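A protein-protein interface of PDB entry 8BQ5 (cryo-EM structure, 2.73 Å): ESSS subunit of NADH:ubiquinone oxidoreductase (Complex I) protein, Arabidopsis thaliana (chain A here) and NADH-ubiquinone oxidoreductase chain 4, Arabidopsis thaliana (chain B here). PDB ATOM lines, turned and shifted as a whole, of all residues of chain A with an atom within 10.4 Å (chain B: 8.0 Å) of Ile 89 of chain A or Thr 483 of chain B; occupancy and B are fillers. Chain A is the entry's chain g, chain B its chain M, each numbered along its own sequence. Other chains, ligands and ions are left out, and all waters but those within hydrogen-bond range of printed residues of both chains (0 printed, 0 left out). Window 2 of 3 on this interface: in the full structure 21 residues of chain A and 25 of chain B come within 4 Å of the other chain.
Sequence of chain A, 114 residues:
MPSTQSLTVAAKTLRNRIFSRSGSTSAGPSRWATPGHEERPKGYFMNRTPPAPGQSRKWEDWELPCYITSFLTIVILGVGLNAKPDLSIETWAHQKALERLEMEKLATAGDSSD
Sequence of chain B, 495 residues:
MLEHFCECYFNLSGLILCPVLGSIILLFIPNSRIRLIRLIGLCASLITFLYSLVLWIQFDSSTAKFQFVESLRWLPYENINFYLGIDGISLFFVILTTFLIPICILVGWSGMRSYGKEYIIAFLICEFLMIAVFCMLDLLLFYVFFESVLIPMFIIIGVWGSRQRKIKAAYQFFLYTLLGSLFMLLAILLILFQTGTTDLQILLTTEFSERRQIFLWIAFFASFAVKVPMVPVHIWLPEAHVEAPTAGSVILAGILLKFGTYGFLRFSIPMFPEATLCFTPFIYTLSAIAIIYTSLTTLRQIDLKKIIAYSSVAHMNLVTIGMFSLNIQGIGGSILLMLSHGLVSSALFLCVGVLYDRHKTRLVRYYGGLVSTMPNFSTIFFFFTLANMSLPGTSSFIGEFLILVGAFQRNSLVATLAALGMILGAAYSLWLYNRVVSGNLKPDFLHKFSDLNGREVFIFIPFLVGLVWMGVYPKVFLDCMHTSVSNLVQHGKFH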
ATOM      1  N   PRO A  85       8.244 -12.456  11.014  1.00  0.00           N
ATOM      2  CA  PRO A  85       9.476 -11.675  11.168  1.00  0.00           C
ATOM      3  C   PRO A  85      10.445 -12.348  12.126  1.00  0.00           C
ATOM      4  O   PRO A  85      10.046 -13.030  13.071  1.00  0.00           O
ATOM      5  CB  PRO A  85       8.978 -10.336  11.722  1.00  0.00           C
ATOM      6  CG  PRO A  85       7.703 -10.672  12.409  1.00  0.00           C
ATOM      7  CD  PRO A  85       7.080 -11.776  11.607  1.00  0.00           C
ATOM      8  N   ASP A  86      11.735 -12.152  11.868  1.00  0.00           N
ATOM      9  CA  ASP A  86      12.774 -12.685  12.740  1.00  0.00           C
ATOM     10  C   ASP A  86      12.940 -11.750  13.929  1.00  0.00           C
ATOM     11  O   ASP A  86      13.759 -10.825  13.896  1.00  0.00           O
ATOM     12  CB  ASP A  86      14.088 -12.853  11.985  1.00  0.00           C
ATOM     13  CG  ASP A  86      14.988 -13.892  12.622  1.00  0.00           C
ATOM     14  OD1 ASP A  86      15.377 -13.703  13.793  1.00  0.00           O
ATOM     15  OD2 ASP A  86      15.291 -14.902  11.958  1.00  0.00           O
ATOM     16  N   LEU A  87      12.163 -11.992  14.983  1.00  0.00           N
ATOM     17  CA  LEU A  87      12.184 -11.168  16.182  1.00  0.00           C
ATOM     18  C   LEU A  87      12.964 -11.821  17.315  1.00  0.00           C
ATOM     19  O   LEU A  87      12.852 -11.392  18.465  1.00  0.00           O
ATOM     20  CB  LEU A  87      10.756 -10.853  16.628  1.00  0.00           C
ATOM     21  CG  LEU A  87       9.846 -10.346  15.508  1.00  0.00           C
ATOM     22  CD1 LEU A  87       8.405 -10.244  15.978  1.00  0.00           C
ATOM     23  CD2 LEU A  87      10.341  -9.008  14.976  1.00  0.00           C
ATOM     24  N   SER A  88      13.754 -12.848  17.013  1.00  0.00           N
ATOM     25  CA  SER A  88      14.532 -13.514  18.048  1.00  0.00           C
ATOM     26  C   SER A  88      15.527 -12.545  18.675  1.00  0.00           C
ATOM     27  O   SER A  88      16.045 -11.636  18.018  1.00  0.00           O
ATOM     28  CB  SER A  88      15.262 -14.724  17.468  1.00  0.00           C
ATOM     29  OG  SER A  88      16.309 -14.319  16.605  1.00  0.00           O
ATOM     30  N   ILE A  89      15.783 -12.740  19.972  1.00  0.00           N
ATOM     31  CA  ILE A  89      16.683 -11.850  20.703  1.00  0.00           C
ATOM     32  C   ILE A  89      18.078 -11.877  20.100  1.00  0.00           C
ATOM     33  O   ILE A  89      18.752 -10.842  20.028  1.00  0.00           O
ATOM     34  CB  ILE A  89      16.705 -12.221  22.201  1.00  0.00           C
ATOM     35  CG1 ILE A  89      17.812 -11.462  22.931  1.00  0.00           C
ATOM     36  CG2 ILE A  89      16.877 -13.723  22.387  1.00  0.00           C
ATOM     37  CD1 ILE A  89      17.496 -10.011  23.184  1.00  0.00           C
ATOM     38  N   GLU A  90      18.527 -13.047  19.644  1.00  0.00           N
ATOM     39  CA  GLU A  90      19.868 -13.166  19.081  1.00  0.00           C
ATOM     40  C   GLU A  90      20.037 -12.271  17.858  1.00  0.00           C
ATOM     41  O   GLU A  90      21.062 -11.600  17.705  1.00  0.00           O
ATOM     42  CB  GLU A  90      20.153 -14.627  18.732  1.00  0.00           C
ATOM     43  CG  GLU A  90      19.962 -15.589  19.898  1.00  0.00           C
ATOM     44  CD  GLU A  90      18.691 -16.416  19.792  1.00  0.00           C
ATOM     45  OE1 GLU A  90      18.682 -17.558  20.295  1.00  0.00           O
ATOM     46  OE2 GLU A  90      17.700 -15.928  19.212  1.00  0.00           O
ATOM     47  N   THR A  91      19.034 -12.238  16.979  1.00  0.00           N
ATOM     48  CA  THR A  91      19.129 -11.392  15.793  1.00  0.00           C
ATOM     49  C   THR A  91      19.222  -9.917  16.172  1.00  0.00           C
ATOM     50  O   THR A  91      19.988  -9.161  15.564  1.00  0.00           O
ATOM     51  CB  THR A  91      17.932 -11.634  14.876  1.00  0.00           C
ATOM     52  OG1 THR A  91      17.868 -13.023  14.531  1.00  0.00           O
ATOM     53  CG2 THR A  91      18.063 -10.814  13.603  1.00  0.00           C
ATOM     54  N   TRP A  92      18.442  -9.490  17.169  1.00  0.00           N
ATOM     55  CA  TRP A  92      18.494  -8.099  17.607  1.00  0.00           C
ATOM     56  C   TRP A  92      19.842  -7.756  18.228  1.00  0.00           C
ATOM     57  O   TRP A  92      20.410  -6.695  17.945  1.00  0.00           O
ATOM     58  CB  TRP A  92      17.363  -7.821  18.599  1.00  0.00           C
ATOM     59  CG  TRP A  92      17.465  -6.482  19.270  1.00  0.00           C
ATOM     60  CD1 TRP A  92      16.902  -5.315  18.854  1.00  0.00           C
ATOM     61  CD2 TRP A  92      18.163  -6.178  20.485  1.00  0.00           C
ATOM     62  NE1 TRP A  92      17.212  -4.300  19.725  1.00  0.00           N
ATOM     63  CE2 TRP A  92      17.985  -4.805  20.737  1.00  0.00           C
ATOM     64  CE3 TRP A  92      18.924  -6.934  21.382  1.00  0.00           C
ATOM     65  CZ2 TRP A  92      18.538  -4.172  21.846  1.00  0.00           C
ATOM     66  CZ3 TRP A  92      19.476  -6.303  22.479  1.00  0.00           C
ATOM     67  CH2 TRP A  92      19.278  -4.936  22.704  1.00  0.00           C
ATOM     68  N   ALA A  93      20.369  -8.639  19.080  1.00  0.00           N
ATOM     69  CA  ALA A  93      21.621  -8.346  19.769  1.00  0.00           C
ATOM     70  C   ALA A  93      22.813  -8.396  18.827  1.00  0.00           C
ATOM     71  O   ALA A  93      23.806  -7.696  19.052  1.00  0.00           O
ATOM     72  CB  ALA A  93      21.825  -9.316  20.931  1.00  0.00           C
ATOM     73  N   HIS A  94      22.747  -9.220  17.782  1.00  0.00           N
ATOM     74  CA  HIS A  94      23.841  -9.274  16.818  1.00  0.00           C
ATOM     75  C   HIS A  94      23.987  -7.947  16.085  1.00  0.00           C
ATOM     76  O   HIS A  94      25.104  -7.464  15.866  1.00  0.00           O
ATOM     77  CB  HIS A  94      23.616 -10.415  15.831  1.00  0.00           C
ATOM     78  CG  HIS A  94      24.720 -10.569  14.835  1.00  0.00           C
ATOM     79  ND1 HIS A  94      25.819 -11.369  15.061  1.00  0.00           N
ATOM     80  CD2 HIS A  94      24.897 -10.025  13.608  1.00  0.00           C
ATOM     81  CE1 HIS A  94      26.624 -11.310  14.016  1.00  0.00           C
ATOM     82  NE2 HIS A  94      26.088 -10.502  13.121  1.00  0.00           N
ATOM     83  N   GLN A  95      22.864  -7.347  15.686  1.00  0.00           N
ATOM     84  CA  GLN A  95      22.917  -6.023  15.077  1.00  0.00           C
ATOM     85  C   GLN A  95      23.413  -4.982  16.069  1.00  0.00           C
ATOM     86  O   GLN A  95      24.214  -4.109  15.715  1.00  0.00           O
ATOM     87  CB  GLN A  95      21.541  -5.638  14.534  1.00  0.00           C
ATOM     88  CG  GLN A  95      21.571  -4.964  13.172  1.00  0.00           C
ATOM     89  CD  GLN A  95      21.916  -5.917  12.043  1.00  0.00           C
ATOM     90  OE1 GLN A  95      22.250  -7.081  12.270  1.00  0.00           O
ATOM     91  NE2 GLN A  95      21.828  -5.427  10.812  1.00  0.00           N
ATOM     92  N   LYS A  96      22.951  -5.060  17.317  1.00  0.00           N
ATOM     93  CA  LYS A  96      23.387  -4.107  18.331  1.00  0.00           C
ATOM     94  C   LYS A  96      24.865  -4.284  18.660  1.00  0.00           C
ATOM     95  O   LYS A  96      25.555  -3.312  18.981  1.00  0.00           O
ATOM     96  CB  LYS A  96      22.534  -4.259  19.588  1.00  0.00           C
ATOM     97  CG  LYS A  96      21.176  -3.578  19.510  1.00  0.00           C
ATOM     98  CD  LYS A  96      21.270  -2.090  19.803  1.00  0.00           C
ATOM     99  CE  LYS A  96      20.024  -1.356  19.334  1.00  0.00           C
ATOM    100  NZ  LYS A  96      19.526  -1.868  18.029  1.00  0.00           N
ATOM    101  N   ALA A  97      25.365  -5.520  18.596  1.00  0.00           N
ATOM    102  CA  ALA A  97      26.775  -5.766  18.881  1.00  0.00           C
ATOM    103  C   ALA A  97      27.664  -5.235  17.763  1.00  0.00           C
ATOM    104  O   ALA A  97      28.791  -4.790  18.012  1.00  0.00           O
ATOM    105  CB  ALA A  97      27.020  -7.259  19.095  1.00  0.00           C
ATOM    106  N   PHE B  59       3.408 -15.658  17.246  1.00  0.00           N
ATOM    107  CA  PHE B  59       4.180 -15.554  18.474  1.00  0.00           C
ATOM    108  C   PHE B  59       5.330 -14.565  18.314  1.00  0.00           C
ATOM    109  O   PHE B  59       5.991 -14.523  17.273  1.00  0.00           O
ATOM    110  CB  PHE B  59       4.720 -16.929  18.868  1.00  0.00           C
ATOM    111  CG  PHE B  59       5.420 -16.954  20.191  1.00  0.00           C
ATOM    112  CD1 PHE B  59       4.699 -16.985  21.371  1.00  0.00           C
ATOM    113  CD2 PHE B  59       6.803 -16.959  20.253  1.00  0.00           C
ATOM    114  CE1 PHE B  59       5.344 -17.016  22.588  1.00  0.00           C
ATOM    115  CE2 PHE B  59       7.453 -16.988  21.467  1.00  0.00           C
ATOM    116  CZ  PHE B  59       6.724 -17.015  22.636  1.00  0.00           C
ATOM    117  N   ASP B  60       5.564 -13.770  19.356  1.00  0.00           N
ATOM    118  CA  ASP B  60       6.655 -12.799  19.394  1.00  0.00           C
ATOM    119  C   ASP B  60       7.782 -13.412  20.218  1.00  0.00           C
ATOM    120  O   ASP B  60       7.594 -13.736  21.395  1.00  0.00           O
ATOM    121  CB  ASP B  60       6.180 -11.470  19.984  1.00  0.00           C
ATOM    122  CG  ASP B  60       7.270 -10.398  20.015  1.00  0.00           C
ATOM    123  OD1 ASP B  60       8.476 -10.724  20.015  1.00  0.00           O
ATOM    124  OD2 ASP B  60       6.909  -9.205  20.040  1.00  0.00           O
ATOM    125  N   SER B  61       8.953 -13.554  19.602  1.00  0.00           N
ATOM    126  CA  SER B  61      10.112 -14.149  20.250  1.00  0.00           C
ATOM    127  C   SER B  61      11.088 -13.106  20.787  1.00  0.00           C
ATOM    128  O   SER B  61      12.191 -13.464  21.214  1.00  0.00           O
ATOM    129  CB  SER B  61      10.819 -15.101  19.283  1.00  0.00           C
ATOM    130  OG  SER B  61      11.441 -14.391  18.229  1.00  0.00           O
ATOM    131  N   SER B  62      10.707 -11.827  20.776  1.00  0.00           N
ATOM    132  CA  SER B  62      11.518 -10.770  21.360  1.00  0.00           C
ATOM    133  C   SER B  62      11.083 -10.371  22.759  1.00  0.00           C
ATOM    134  O   SER B  62      11.916  -9.888  23.530  1.00  0.00           O
ATOM    135  CB  SER B  62      11.494  -9.516  20.474  1.00  0.00           C
ATOM    136  OG  SER B  62      10.268  -8.817  20.614  1.00  0.00           O
ATOM    137  N   THR B  63       9.832 -10.655  23.098  1.00  0.00           N
ATOM    138  CA  THR B  63       9.307 -10.139  24.381  1.00  0.00           C
ATOM    139  C   THR B  63       9.450 -11.118  25.544  1.00  0.00           C
ATOM    140  O   THR B  63       9.506 -12.340  25.306  1.00  0.00           O
ATOM    141  CB  THR B  63       7.853  -9.683  24.207  1.00  0.00           C
ATOM    142  OG1 THR B  63       7.532  -8.836  25.310  1.00  0.00           O
ATOM    143  CG2 THR B  63       6.864 -10.823  24.128  1.00  0.00           C
ATOM    144  N   ALA B  64       9.498 -10.576  26.758  1.00  0.00           N
ATOM    145  CA  ALA B  64       9.512 -11.412  27.974  1.00  0.00           C
ATOM    146  C   ALA B  64       8.138 -11.287  28.631  1.00  0.00           C
ATOM    147  O   ALA B  64       7.908 -11.940  29.659  1.00  0.00           O
ATOM    148  CB  ALA B  64      10.596 -10.912  28.880  1.00  0.00           C
ATOM    149  N   LYS B  65       7.261 -10.465  28.049  1.00  0.00           N
ATOM    150  CA  LYS B  65       5.923 -10.222  28.633  1.00  0.00           C
ATOM    151  C   LYS B  65       5.000 -11.358  28.190  1.00  0.00           C
ATOM    152  O   LYS B  65       5.174 -11.868  27.064  1.00  0.00           O
ATOM    153  CB  LYS B  65       5.419  -8.839  28.206  1.00  0.00           C
ATOM    154  CG  LYS B  65       5.787  -7.697  29.140  1.00  0.00           C
ATOM    155  CD  LYS B  65       7.099  -7.031  28.786  1.00  0.00           C
ATOM    156  CE  LYS B  65       7.353  -5.771  29.585  1.00  0.00           C
ATOM    157  NZ  LYS B  65       6.187  -4.859  29.572  1.00  0.00           N
ATOM    158  N   GLN B  67       2.221 -13.315  26.512  1.00  0.00           N
ATOM    159  CA  GLN B  67       1.605 -12.946  25.222  1.00  0.00           C
ATOM    160  C   GLN B  67       0.157 -13.408  25.157  1.00  0.00           C
ATOM    161  O   GLN B  67      -0.218 -14.283  25.958  1.00  0.00           O
ATOM    162  CB  GLN B  67       2.416 -13.538  24.080  1.00  0.00           C
ATOM    163  CG  GLN B  67       3.697 -12.768  23.838  1.00  0.00           C
ATOM    164  CD  GLN B  67       4.590 -13.532  22.904  1.00  0.00           C
ATOM    165  OE1 GLN B  67       4.241 -13.772  21.754  1.00  0.00           O
ATOM    166  NE2 GLN B  67       5.744 -13.934  23.407  1.00  0.00           N
ATOM    167  N   ASP B  87       3.934 -18.011  27.056  1.00  0.00           N
ATOM    168  CA  ASP B  87       5.237 -17.417  26.784  1.00  0.00           C
ATOM    169  C   ASP B  87       6.040 -18.425  25.972  1.00  0.00           C
ATOM    170  O   ASP B  87       5.485 -19.389  25.436  1.00  0.00           O
ATOM    171  CB  ASP B  87       5.944 -17.021  28.091  1.00  0.00           C
ATOM    172  CG  ASP B  87       5.788 -18.067  29.174  1.00  0.00           C
ATOM    173  OD1 ASP B  87       6.819 -18.595  29.645  1.00  0.00           O
ATOM    174  OD2 ASP B  87       4.638 -18.367  29.550  1.00  0.00           O
ATOM    175  N   GLY B  88       7.347 -18.209  25.882  1.00  0.00           N
ATOM    176  CA  GLY B  88       8.207 -19.162  25.222  1.00  0.00           C
ATOM    177  C   GLY B  88       8.322 -20.500  25.909  1.00  0.00           C
ATOM    178  O   GLY B  88       8.750 -21.473  25.286  1.00  0.00           O
ATOM    179  N   ILE B  89       7.941 -20.585  27.182  1.00  0.00           N
ATOM    180  CA  ILE B  89       8.060 -21.823  27.929  1.00  0.00           C
ATOM    181  C   ILE B  89       6.849 -22.737  27.747  1.00  0.00           C
ATOM    182  O   ILE B  89       7.013 -23.961  27.721  1.00  0.00           O
ATOM    183  CB  ILE B  89       8.312 -21.530  29.425  1.00  0.00           C
ATOM    184  CG1 ILE B  89       9.718 -20.972  29.629  1.00  0.00           C
ATOM    185  CG2 ILE B  89       8.187 -22.787  30.264  1.00  0.00           C
ATOM    186  CD1 ILE B  89       9.770 -19.820  30.601  1.00  0.00           C
ATOM    187  N   ILE B 328      21.277 -21.067  30.359  1.00  0.00           N
ATOM    188  CA  ILE B 328      20.528 -21.164  29.110  1.00  0.00           C
ATOM    189  C   ILE B 328      20.517 -22.597  28.592  1.00  0.00           C
ATOM    190  O   ILE B 328      19.476 -23.111  28.172  1.00  0.00           O
ATOM    191  CB  ILE B 328      21.092 -20.187  28.064  1.00  0.00           C
ATOM    192  CG1 ILE B 328      21.208 -18.784  28.661  1.00  0.00           C
ATOM    193  CG2 ILE B 328      20.217 -20.177  26.824  1.00  0.00           C
ATOM    194  CD1 ILE B 328      19.879 -18.157  29.023  1.00  0.00           C
ATOM    195  N   LEU B 478      14.275 -23.297  19.636  1.00  0.00           N
ATOM    196  CA  LEU B 478      15.134 -22.508  20.514  1.00  0.00           C
ATOM    197  C   LEU B 478      14.992 -21.011  20.255  1.00  0.00           C
ATOM    198  O   LEU B 478      15.193 -20.206  21.170  1.00  0.00           O
ATOM    199  CB  LEU B 478      16.588 -22.949  20.347  1.00  0.00           C
ATOM    200  CG  LEU B 478      16.958 -24.308  20.954  1.00  0.00           C
ATOM    201  CD1 LEU B 478      18.338 -24.753  20.497  1.00  0.00           C
ATOM    202  CD2 LEU B 478      16.896 -24.260  22.471  1.00  0.00           C
ATOM    203  N   ASP B 479      14.650 -20.622  19.024  1.00  0.00           N
ATOM    204  CA  ASP B 479      14.447 -19.207  18.724  1.00  0.00           C
ATOM    205  C   ASP B 479      13.261 -18.636  19.490  1.00  0.00           C
ATOM    206  O   ASP B 479      13.319 -17.502  19.979  1.00  0.00           O
ATOM    207  CB  ASP B 479      14.246 -19.011  17.224  1.00  0.00           C
ATOM    208  CG  ASP B 479      15.551 -18.874  16.478  1.00  0.00           C
ATOM    209  OD1 ASP B 479      16.607 -18.813  17.141  1.00  0.00           O
ATOM    210  OD2 ASP B 479      15.522 -18.830  15.231  1.00  0.00           O
ATOM    211  N   CYS B 480      12.174 -19.399  19.594  1.00  0.00           N
ATOM    212  CA  CYS B 480      10.966 -18.920  20.249  1.00  0.00           C
ATOM    213  C   CYS B 480      11.002 -19.075  21.761  1.00  0.00           C
ATOM    214  O   CYS B 480      10.057 -18.649  22.432  1.00  0.00           O
ATOM    215  CB  CYS B 480       9.742 -19.653  19.695  1.00  0.00           C
ATOM    216  SG  CYS B 480       9.454 -19.413  17.926  1.00  0.00           S
ATOM    217  N   MET B 481      12.055 -19.672  22.315  1.00  0.00           N
ATOM    218  CA  MET B 481      12.125 -19.919  23.749  1.00  0.00           C
ATOM    219  C   MET B 481      13.156 -19.069  24.469  1.00  0.00           C
ATOM    220  O   MET B 481      13.040 -18.884  25.682  1.00  0.00           O
ATOM    221  CB  MET B 481      12.443 -21.395  24.019  1.00  0.00           C
ATOM    222  CG  MET B 481      11.297 -22.353  23.748  1.00  0.00           C
ATOM    223  SD  MET B 481      11.822 -24.072  23.588  1.00  0.00           S
ATOM    224  CE  MET B 481      13.585 -23.928  23.863  1.00  0.00           C
ATOM    225  N   HIS B 482      14.144 -18.530  23.754  1.00  0.00           N
ATOM    226  CA  HIS B 482      15.344 -18.020  24.409  1.00  0.00           C
ATOM    227  C   HIS B 482      15.070 -16.778  25.249  1.00  0.00           C
ATOM    228  O   HIS B 482      15.679 -16.599  26.309  1.00  0.00           O
ATOM    229  CB  HIS B 482      16.426 -17.739  23.370  1.00  0.00           C
ATOM    230  CG  HIS B 482      17.369 -18.882  23.172  1.00  0.00           C
ATOM    231  ND1 HIS B 482      17.971 -19.155  21.964  1.00  0.00           N
ATOM    232  CD2 HIS B 482      17.800 -19.836  24.032  1.00  0.00           C
ATOM    233  CE1 HIS B 482      18.739 -20.222  22.089  1.00  0.00           C
ATOM    234  NE2 HIS B 482      18.654 -20.654  23.334  1.00  0.00           N
ATOM    235  N   THR B 483      14.179 -15.898  24.790  1.00  0.00           N
ATOM    236  CA  THR B 483      13.888 -14.688  25.556  1.00  0.00           C
ATOM    237  C   THR B 483      13.184 -15.021  26.867  1.00  0.00           C
ATOM    238  O   THR B 483      13.520 -14.475  27.923  1.00  0.00           O
ATOM    239  CB  THR B 483      13.048 -13.720  24.723  1.00  0.00           C
ATOM    240  OG1 THR B 483      13.791 -13.312  23.570  1.00  0.00           O
ATOM    241  CG2 THR B 483      12.697 -12.491  25.542  1.00  0.00           C
ATOM    242  N   SER B 484      12.193 -15.916  26.816  1.00  0.00           N
ATOM    243  CA  SER B 484      11.524 -16.351  28.038  1.00  0.00           C
ATOM    244  C   SER B 484      12.474 -17.140  28.927  1.00  0.00           C
ATOM    245  O   SER B 484      12.424 -17.039  30.158  1.00  0.00           O
ATOM    246  CB  SER B 484      10.293 -17.190  27.696  1.00  0.00           C
ATOM    247  OG  SER B 484       9.303 -16.415  27.048  1.00  0.00           O
ATOM    248  N   VAL B 485      13.336 -17.955  28.316  1.00  0.00           N
ATOM    249  CA  VAL B 485      14.308 -18.723  29.087  1.00  0.00           C
ATOM    250  C   VAL B 485      15.318 -17.793  29.746  1.00  0.00           C
ATOM    251  O   VAL B 485      15.666 -17.963  30.920  1.00  0.00           O
ATOM    252  CB  VAL B 485      14.995 -19.767  28.188  1.00  0.00           C
ATOM    253  CG1 VAL B 485      16.284 -20.256  28.824  1.00  0.00           C
ATOM    254  CG2 VAL B 485      14.058 -20.929  27.925  1.00  0.00           C
ATOM    255  N   SER B 486      15.799 -16.794  29.001  1.00  0.00           N
ATOM    256  CA  SER B 486      16.782 -15.863  29.544  1.00  0.00           C
ATOM    257  C   SER B 486      16.223 -15.107  30.739  1.00  0.00           C
ATOM    258  O   SER B 486      16.911 -14.935  31.752  1.00  0.00           O
ATOM    259  CB  SER B 486      17.223 -14.877  28.462  1.00  0.00           C
ATOM    260  OG  SER B 486      18.102 -15.489  27.543  1.00  0.00           O
ATOM    261  N   ASN B 487      14.977 -14.644  30.637  1.00  0.00           N
ATOM    262  CA  ASN B 487      14.368 -13.897  31.728  1.00  0.00           C
ATOM    263  C   ASN B 487      14.048 -14.797  32.912  1.00  0.00           C
ATOM    264  O   ASN B 487      13.971 -14.319  34.050  1.00  0.00           O
ATOM    265  CB  ASN B 487      13.108 -13.193  31.235  1.00  0.00           C
ATOM    266  CG  ASN B 487      13.382 -11.781  30.775  1.00  0.00           C
ATOM    267  OD1 ASN B 487      13.757 -11.554  29.628  1.00  0.00           O
ATOM    268  ND2 ASN B 487      13.198 -10.822  31.666  1.00  0.00           N
ATOM    269  N   LEU B 488      13.868 -16.094  32.660  1.00  0.00           N
ATOM    270  CA  LEU B 488      13.646 -17.048  33.779  1.00  0.00           C
ATOM    271  C   LEU B 488      14.955 -17.189  34.563  1.00  0.00           C
ATOM    272  O   LEU B 488      14.899 -17.185  35.808  1.00  0.00           O
ATOM    273  CB  LEU B 488      13.186 -18.387  33.196  1.00  0.00           C
ATOM    274  CG  LEU B 488      13.113 -19.563  34.167  1.00  0.00           C
ATOM    275  CD1 LEU B 488      12.090 -19.300  35.259  1.00  0.00           C
ATOM    276  CD2 LEU B 488      12.772 -20.843  33.426  1.00  0.00           C
ATOM    277  N   VAL B 489      16.089 -17.278  33.860  1.00  0.00           N
ATOM    278  CA  VAL B 489      17.368 -17.465  34.533  1.00  0.00           C
ATOM    279  C   VAL B 489      17.774 -16.199  35.279  1.00  0.00           C
ATOM    280  O   VAL B 489      18.312 -16.261  36.391  1.00  0.00           O
ATOM    281  CB  VAL B 489      18.435 -17.900  33.512  1.00  0.00           C
ATOM    282  CG1 VAL B 489      19.819 -17.782  34.102  1.00  0.00           C
ATOM    283  CG2 VAL B 489      18.175 -19.324  33.043  1.00  0.00           C
ATOM    284  N   GLN B 490      17.516 -15.032  34.687  1.00  0.00           N
ATOM    285  CA  GLN B 490      17.928 -13.766  35.279  1.00  0.00           C
ATOM    286  C   GLN B 490      17.042 -13.333  36.440  1.00  0.00           C
ATOM    287  O   GLN B 490      17.447 -12.465  37.221  1.00  0.00           O
ATOM    288  CB  GLN B 490      17.940 -12.674  34.210  1.00  0.00           C
ATOM    289  CG  GLN B 490      18.526 -11.361  34.675  1.00  0.00           C
ATOM    290  CD  GLN B 490      20.030 -11.428  34.769  1.00  0.00           C
ATOM    291  OE1 GLN B 490      20.726 -11.355  33.760  1.00  0.00           O
ATOM    292  NE2 GLN B 490      20.543 -11.577  35.985  1.00  0.00           N
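The side-chain hydroxyl (OG) of Ser 61 of chain B lies within hydrogen-bond range of the backbone NH (N) of Ser 88 of chain A, at 3.0 Å. The side-chain hydroxyl (OG) of Ser 61 of chain B sits close to the backbone carbonyl oxygen (O) of Leu 87 of chain A (3.3 Å). A ring nitrogen (ND1) of His 482 of chain B sits at hydrogen-bond distance from the side-chain carboxylate (OE1) of Glu 90 of chain A, at 2.4 Å. The backbone carbonyl oxygen (O) of Leu 87 of chain A lies close to the backbone NH (N) of Ser 62 of chain B (3.2 Å).
O of Ser 61 of chain B lies within hydrogen-bond range of OG1 of Thr 483 of chain B, 2.9 Å away. The side-chain carboxylate (OD1) of Asp 86 of chain A is in hydrogen-bond range of the side-chain hydroxyl (OG) of Ser 88 of chain A (3.0 Å). The side-chain hydroxyl of Thr 91 of chain A sits at hydrogen-bond distance from the side-chain hydroxyl of Ser 88 of chain A (2.9 Å). O of His 482 of chain B lies within hydrogen-bond range of OG of Ser 486 of chain B. The side-chain carboxylate (OD1) of Asp 60 of chain B is in hydrogen-bond range of the backbone NH (N) of Ser 62 of chain B (2.6 Å). O of Leu 478 of chain B sits at hydrogen-bond distance from ND1 of His 482 of chain B, 3.1 Å away.
Ser 61 of chain B touches Ile 89 of chain A (O to N, 3.9 Å). Ile 89 of chain A touches Thr 483 of chain B (CG2 to OG1, 3.3 Å). Asp 479 of chain B touches Glu 90 of chain A.
Pro 85 of chain A touches none of the printed residues of chain B. Printed residues of chain B within 4 Å of Leu 87 of chain A: Ser 61 and Ser 62. Ser 88 of chain A touches just one residue of chain B: Ser 61. Of chain B, only Ser 61 (3.9 Å) and Thr 483 (3.3 Å) come within 4 Å of Ile 89 of chain A. Ser 61 of chain B touches just these residues of chain A: Leu 87, Ser 88 and Ile 89. Printed residues of chain A within 4 Å of Ser 62 of chain B: Leu 87. Thr 63 of chain B touches none of the printed residues of chain A. Ile 89 of chain B touches none of the printed residues of chain A. Of the printed residues of chain A, Thr 483 of chain B touches Ile 89 (3.3 Å). No residue of chain A comes within 4 Å of Ser 484 of chain B. No residue of chain A comes within 4 Å of Val 485 of chain B. No residue of chain A comes within 4 Å of Ser 486 of chain B. No residue of chain A comes within 4 Å of Asn 487 of chain B. The nearest residue of chain B that does not touch Ile 89 of chain A is His 482 of chain B (4.2 Å). The nearest residue of chain A that does not touch Thr 483 of chain B is Ser 88 of chain A (5.3 Å).
Of the 25 printed residues of chain B, 5 touch a printed residue of chain A. Hydrophobic or aromatic side chains of chain B that line the printed part of chain A: His 482.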
